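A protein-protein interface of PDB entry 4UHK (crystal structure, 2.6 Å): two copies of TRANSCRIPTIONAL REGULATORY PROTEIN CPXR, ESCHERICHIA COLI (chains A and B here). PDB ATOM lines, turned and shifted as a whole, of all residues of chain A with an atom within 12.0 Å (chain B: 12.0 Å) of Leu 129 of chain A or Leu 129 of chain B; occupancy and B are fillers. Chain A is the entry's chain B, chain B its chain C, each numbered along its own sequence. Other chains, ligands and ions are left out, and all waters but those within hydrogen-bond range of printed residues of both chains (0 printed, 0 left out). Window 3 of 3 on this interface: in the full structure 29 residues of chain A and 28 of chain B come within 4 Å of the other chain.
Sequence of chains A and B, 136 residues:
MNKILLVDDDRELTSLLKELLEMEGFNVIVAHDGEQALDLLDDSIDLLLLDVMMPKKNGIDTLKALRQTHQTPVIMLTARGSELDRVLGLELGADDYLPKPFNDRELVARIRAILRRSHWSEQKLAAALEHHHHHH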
ATOM      1  N   TRP A 120      22.713   1.766 -34.401  1.00  0.00           N
ATOM      2  CA  TRP A 120      23.969   2.152 -35.033  1.00  0.00           C
ATOM      3  C   TRP A 120      25.017   2.507 -33.987  1.00  0.00           C
ATOM      4  O   TRP A 120      26.181   2.126 -34.139  1.00  0.00           O
ATOM      5  CB  TRP A 120      23.767   3.329 -35.982  1.00  0.00           C
ATOM      6  CG  TRP A 120      23.171   2.982 -37.323  1.00  0.00           C
ATOM      7  CD1 TRP A 120      23.218   1.777 -37.967  1.00  0.00           C
ATOM      8  CD2 TRP A 120      22.534   3.890 -38.223  1.00  0.00           C
ATOM      9  NE1 TRP A 120      22.619   1.874 -39.198  1.00  0.00           N
ATOM     10  CE2 TRP A 120      22.194   3.161 -39.386  1.00  0.00           C
ATOM     11  CE3 TRP A 120      22.193   5.246 -38.151  1.00  0.00           C
ATOM     12  CZ2 TRP A 120      21.516   3.739 -40.461  1.00  0.00           C
ATOM     13  CZ3 TRP A 120      21.537   5.824 -39.222  1.00  0.00           C
ATOM     14  CH2 TRP A 120      21.195   5.073 -40.357  1.00  0.00           C
ATOM     15  N   SER A 121      24.582   3.213 -32.913  1.00  0.00           N
ATOM     16  CA  SER A 121      25.377   3.642 -31.754  1.00  0.00           C
ATOM     17  C   SER A 121      25.886   2.438 -30.963  1.00  0.00           C
ATOM     18  O   SER A 121      27.042   2.439 -30.532  1.00  0.00           O
ATOM     19  CB  SER A 121      24.541   4.541 -30.850  1.00  0.00           C
ATOM     20  OG  SER A 121      24.368   5.829 -31.421  1.00  0.00           O
ATOM     21  N   GLU A 122      25.023   1.413 -30.782  1.00  0.00           N
ATOM     22  CA  GLU A 122      25.329   0.149 -30.098  1.00  0.00           C
ATOM     23  C   GLU A 122      26.315  -0.676 -30.928  1.00  0.00           C
ATOM     24  O   GLU A 122      27.283  -1.190 -30.368  1.00  0.00           O
ATOM     25  CB  GLU A 122      24.043  -0.660 -29.844  1.00  0.00           C
ATOM     26  CG  GLU A 122      23.136  -0.084 -28.768  1.00  0.00           C
ATOM     27  CD  GLU A 122      21.678  -0.517 -28.783  1.00  0.00           C
ATOM     28  OE1 GLU A 122      21.305  -1.379 -29.615  1.00  0.00           O
ATOM     29  OE2 GLU A 122      20.902   0.021 -27.962  1.00  0.00           O
ATOM     30  N   GLN A 123      26.073  -0.802 -32.261  1.00  0.00           N
ATOM     31  CA  GLN A 123      26.939  -1.525 -33.206  1.00  0.00           C
ATOM     32  C   GLN A 123      28.344  -0.931 -33.216  1.00  0.00           C
ATOM     33  O   GLN A 123      29.315  -1.688 -33.182  1.00  0.00           O
ATOM     34  CB  GLN A 123      26.374  -1.504 -34.639  1.00  0.00           C
ATOM     35  CG  GLN A 123      25.148  -2.371 -34.875  1.00  0.00           C
ATOM     36  CD  GLN A 123      24.896  -2.581 -36.348  1.00  0.00           C
ATOM     37  OE1 GLN A 123      25.252  -3.619 -36.896  1.00  0.00           O
ATOM     38  NE2 GLN A 123      24.269  -1.619 -37.030  1.00  0.00           N
ATOM     39  N   LYS A 124      28.447   0.418 -33.270  1.00  0.00           N
ATOM     40  CA  LYS A 124      29.717   1.144 -33.264  1.00  0.00           C
ATOM     41  C   LYS A 124      30.444   0.902 -31.931  1.00  0.00           C
ATOM     42  O   LYS A 124      31.655   0.645 -31.937  1.00  0.00           O
ATOM     43  CB  LYS A 124      29.501   2.646 -33.519  1.00  0.00           C
ATOM     44  CG  LYS A 124      30.799   3.443 -33.676  1.00  0.00           C
ATOM     45  CD  LYS A 124      30.566   4.881 -34.113  1.00  0.00           C
ATOM     46  CE  LYS A 124      30.211   4.973 -35.579  1.00  0.00           C
ATOM     47  NZ  LYS A 124      29.346   6.150 -35.874  1.00  0.00           N
ATOM     48  N   LEU A 125      29.688   0.935 -30.806  1.00  0.00           N
ATOM     49  CA  LEU A 125      30.197   0.696 -29.453  1.00  0.00           C
ATOM     50  C   LEU A 125      30.742  -0.738 -29.315  1.00  0.00           C
ATOM     51  O   LEU A 125      31.831  -0.915 -28.767  1.00  0.00           O
ATOM     52  CB  LEU A 125      29.094   0.975 -28.407  1.00  0.00           C
ATOM     53  CG  LEU A 125      29.473   0.814 -26.925  1.00  0.00           C
ATOM     54  CD1 LEU A 125      30.409   1.921 -26.458  1.00  0.00           C
ATOM     55  CD2 LEU A 125      28.239   0.794 -26.061  1.00  0.00           C
ATOM     56  N   ALA A 126      29.996  -1.741 -29.834  1.00  0.00           N
ATOM     57  CA  ALA A 126      30.390  -3.156 -29.827  1.00  0.00           C
ATOM     58  C   ALA A 126      31.576  -3.397 -30.763  1.00  0.00           C
ATOM     59  O   ALA A 126      32.423  -4.231 -30.444  1.00  0.00           O
ATOM     60  CB  ALA A 126      29.222  -4.039 -30.230  1.00  0.00           C
ATOM     61  N   ALA A 127      31.648  -2.653 -31.900  1.00  0.00           N
ATOM     62  CA  ALA A 127      32.751  -2.722 -32.872  1.00  0.00           C
ATOM     63  C   ALA A 127      34.041  -2.194 -32.251  1.00  0.00           C
ATOM     64  O   ALA A 127      35.098  -2.805 -32.425  1.00  0.00           O
ATOM     65  CB  ALA A 127      32.412  -1.928 -34.122  1.00  0.00           C
ATOM     66  N   ALA A 128      33.942  -1.078 -31.499  1.00  0.00           N
ATOM     67  CA  ALA A 128      35.064  -0.454 -30.796  1.00  0.00           C
ATOM     68  C   ALA A 128      35.555  -1.332 -29.628  1.00  0.00           C
ATOM     69  O   ALA A 128      36.748  -1.332 -29.326  1.00  0.00           O
ATOM     70  CB  ALA A 128      34.655   0.918 -30.286  1.00  0.00           C
ATOM     71  N   LEU A 129      34.632  -2.091 -29.000  1.00  0.00           N
ATOM     72  CA  LEU A 129      34.904  -2.989 -27.876  1.00  0.00           C
ATOM     73  C   LEU A 129      35.322  -4.378 -28.358  1.00  0.00           C
ATOM     74  O   LEU A 129      36.340  -4.516 -29.033  1.00  0.00           O
ATOM     75  CB  LEU A 129      33.653  -3.094 -26.989  1.00  0.00           C
ATOM     76  CG  LEU A 129      33.614  -2.248 -25.705  1.00  0.00           C
ATOM     77  CD1 LEU A 129      33.771  -0.758 -25.989  1.00  0.00           C
ATOM     78  CD2 LEU A 129      32.322  -2.473 -24.958  1.00  0.00           C
ATOM     79  N   TRP B 120      25.970  12.325 -26.773  1.00  0.00           N
ATOM     80  CA  TRP B 120      25.735  11.322 -25.729  1.00  0.00           C
ATOM     81  C   TRP B 120      26.345   9.970 -26.112  1.00  0.00           C
ATOM     82  O   TRP B 120      26.928   9.292 -25.267  1.00  0.00           O
ATOM     83  CB  TRP B 120      24.236  11.143 -25.472  1.00  0.00           C
ATOM     84  CG  TRP B 120      23.591  12.207 -24.640  1.00  0.00           C
ATOM     85  CD1 TRP B 120      24.196  13.033 -23.739  1.00  0.00           C
ATOM     86  CD2 TRP B 120      22.186  12.497 -24.575  1.00  0.00           C
ATOM     87  NE1 TRP B 120      23.260  13.844 -23.141  1.00  0.00           N
ATOM     88  CE2 TRP B 120      22.016  13.523 -23.620  1.00  0.00           C
ATOM     89  CE3 TRP B 120      21.054  12.010 -25.258  1.00  0.00           C
ATOM     90  CZ2 TRP B 120      20.760  14.068 -23.326  1.00  0.00           C
ATOM     91  CZ3 TRP B 120      19.811  12.550 -24.965  1.00  0.00           C
ATOM     92  CH2 TRP B 120      19.673  13.571 -24.012  1.00  0.00           C
ATOM     93  N   SER B 121      26.209   9.600 -27.403  1.00  0.00           N
ATOM     94  CA  SER B 121      26.717   8.383 -28.039  1.00  0.00           C
ATOM     95  C   SER B 121      28.253   8.358 -28.014  1.00  0.00           C
ATOM     96  O   SER B 121      28.846   7.311 -27.736  1.00  0.00           O
ATOM     97  CB  SER B 121      26.183   8.305 -29.470  1.00  0.00           C
ATOM     98  OG  SER B 121      26.775   7.306 -30.276  1.00  0.00           O
ATOM     99  N   GLU B 122      28.880   9.523 -28.297  1.00  0.00           N
ATOM    100  CA  GLU B 122      30.333   9.730 -28.284  1.00  0.00           C
ATOM    101  C   GLU B 122      30.871   9.660 -26.850  1.00  0.00           C
ATOM    102  O   GLU B 122      31.886   9.000 -26.625  1.00  0.00           O
ATOM    103  CB  GLU B 122      30.701  11.084 -28.917  1.00  0.00           C
ATOM    104  CG  GLU B 122      30.516  11.144 -30.427  1.00  0.00           C
ATOM    105  CD  GLU B 122      30.392  12.521 -31.056  1.00  0.00           C
ATOM    106  OE1 GLU B 122      30.528  13.541 -30.338  1.00  0.00           O
ATOM    107  OE2 GLU B 122      30.138  12.574 -32.282  1.00  0.00           O
ATOM    108  N   GLN B 123      30.192  10.341 -25.886  1.00  0.00           N
ATOM    109  CA  GLN B 123      30.550  10.351 -24.458  1.00  0.00           C
ATOM    110  C   GLN B 123      30.532   8.941 -23.895  1.00  0.00           C
ATOM    111  O   GLN B 123      31.464   8.573 -23.184  1.00  0.00           O
ATOM    112  CB  GLN B 123      29.599  11.234 -23.628  1.00  0.00           C
ATOM    113  CG  GLN B 123      29.749  12.732 -23.824  1.00  0.00           C
ATOM    114  CD  GLN B 123      29.044  13.523 -22.751  1.00  0.00           C
ATOM    115  OE1 GLN B 123      27.806  13.533 -22.625  1.00  0.00           O
ATOM    116  NE2 GLN B 123      29.826  14.297 -22.036  1.00  0.00           N
ATOM    117  N   LYS B 124      29.472   8.152 -24.212  1.00  0.00           N
ATOM    118  CA  LYS B 124      29.318   6.766 -23.766  1.00  0.00           C
ATOM    119  C   LYS B 124      30.447   5.906 -24.359  1.00  0.00           C
ATOM    120  O   LYS B 124      31.040   5.098 -23.639  1.00  0.00           O
ATOM    121  CB  LYS B 124      27.928   6.207 -24.139  1.00  0.00           C
ATOM    122  CG  LYS B 124      27.662   4.817 -23.545  1.00  0.00           C
ATOM    123  CD  LYS B 124      26.279   4.258 -23.833  1.00  0.00           C
ATOM    124  CE  LYS B 124      26.161   2.817 -23.375  1.00  0.00           C
ATOM    125  NZ  LYS B 124      24.788   2.269 -23.539  1.00  0.00           N
ATOM    126  N   LEU B 125      30.762   6.122 -25.659  1.00  0.00           N
ATOM    127  CA  LEU B 125      31.820   5.419 -26.389  1.00  0.00           C
ATOM    128  C   LEU B 125      33.201   5.711 -25.767  1.00  0.00           C
ATOM    129  O   LEU B 125      33.977   4.775 -25.565  1.00  0.00           O
ATOM    130  CB  LEU B 125      31.791   5.803 -27.883  1.00  0.00           C
ATOM    131  CG  LEU B 125      32.808   5.122 -28.802  1.00  0.00           C
ATOM    132  CD1 LEU B 125      32.467   3.667 -29.024  1.00  0.00           C
ATOM    133  CD2 LEU B 125      32.882   5.827 -30.134  1.00  0.00           C
ATOM    134  N   ALA B 126      33.482   6.996 -25.443  1.00  0.00           N
ATOM    135  CA  ALA B 126      34.729   7.434 -24.809  1.00  0.00           C
ATOM    136  C   ALA B 126      34.814   6.927 -23.366  1.00  0.00           C
ATOM    137  O   ALA B 126      35.912   6.598 -22.908  1.00  0.00           O
ATOM    138  CB  ALA B 126      34.833   8.949 -24.841  1.00  0.00           C
ATOM    139  N   ALA B 127      33.658   6.844 -22.658  1.00  0.00           N
ATOM    140  CA  ALA B 127      33.561   6.331 -21.285  1.00  0.00           C
ATOM    141  C   ALA B 127      33.876   4.833 -21.252  1.00  0.00           C
ATOM    142  O   ALA B 127      34.609   4.380 -20.367  1.00  0.00           O
ATOM    143  CB  ALA B 127      32.172   6.589 -20.715  1.00  0.00           C
ATOM    144  N   ALA B 128      33.350   4.077 -22.243  1.00  0.00           N
ATOM    145  CA  ALA B 128      33.577   2.640 -22.394  1.00  0.00           C
ATOM    146  C   ALA B 128      35.035   2.342 -22.787  1.00  0.00           C
ATOM    147  O   ALA B 128      35.577   1.312 -22.381  1.00  0.00           O
ATOM    148  CB  ALA B 128      32.630   2.073 -23.435  1.00  0.00           C
ATOM    149  N   LEU B 129      35.670   3.262 -23.546  1.00  0.00           N
ATOM    150  CA  LEU B 129      37.054   3.159 -24.017  1.00  0.00           C
ATOM    151  C   LEU B 129      38.038   3.717 -22.986  1.00  0.00           C
ATOM    152  O   LEU B 129      38.138   3.192 -21.881  1.00  0.00           O
ATOM    153  CB  LEU B 129      37.199   3.913 -25.351  1.00  0.00           C
ATOM    154  CG  LEU B 129      37.173   3.085 -26.649  1.00  0.00           C
ATOM    155  CD1 LEU B 129      35.893   2.268 -26.794  1.00  0.00           C
ATOM    156  CD2 LEU B 129      37.333   3.980 -27.857  1.00  0.00           C
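The side-chain hydroxyl (OG) of Ser 121 of chain A lies within hydrogen-bond range of the side-chain hydroxyl (OG) of Ser 121 of chain B (3.0 Å).
Among the printed residues, pairs that only touch across the chains: Leu 125 of chain A with Lys 124 of chain B, Leu 125 of chain A with Leu 125 of chain B, Leu 125 of chain A with Ala 128 of chain B, Ala 128 of chain A with Leu 125 of chain B, Ala 128 of chain A with Leu 129 of chain B, Leu 129 of chain A with Ala 128 of chain B and Leu 129 of chain A with Leu 129 of chain B.
Printed residues of chain B within 4 Å of Ser 121 of chain A: Ser 121 (3.0 Å).
Ala 126 of chain A touches none of the printed residues of chain B.
Of the printed residues of chain B, Ala 128 of chain A touches Leu 125 (3.7 Å) and Leu 129 (3.9 Å).
Leu 129 of chain A touches just these residues of chain B: Ala 128 and Leu 129.
Gln 123 of chain B touches none of the printed residues of chain A.
Of the printed residues of chain A, Lys 124 of chain B touches Leu 125.
Leu 125 of chain B touches two residues of chain A.
No residue of chain A comes within 4 Å of Ala 127 of chain B.
Ala 128 of chain B touches just these residues of chain A: Leu 125 and Leu 129.
Leu 129 of chain B touches two residues of chain A.
The nearest residue of chain A that does not touch Leu 129 of chain B is Leu 125 of chain A (5.5 Å).
Of the 10 printed residues of chain B, 5 touch a printed residue of chain A.
Hydrophobic or aromatic side chains of chain B within 4 Å of the printed part of chain A: Leu 125, Ala 128 and Leu 129.
Hydrophobic or aromatic side chains of chain A within 4 Å of the printed part of chain B: Leu 125, Ala 128 and Leu 129.
Ser 121 of chain A touches its own counterpart, Ser 121 of chain B.
Leu 125 of chain A touches Lys 124 of chain B, but with the chains exchanged Lys 124 of chain A does not touch Leu 125 of chain B (4.3 Å).
Leu 125 of chain B touches its own counterpart, Leu 125 of chain A.
Ala 128 of chain A touches Leu 129 of chain B, and with the chains exchanged Leu 129 of chain A touches Ala 128 of chain B.
Positions printed for both chains: 120, 121, 122, 123, 124, 125, 126, 127, 128 and 129.
Of the 8 pairs that touch across the chains among the printed residues, 7 have their exchanged pair printed and touching as well.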
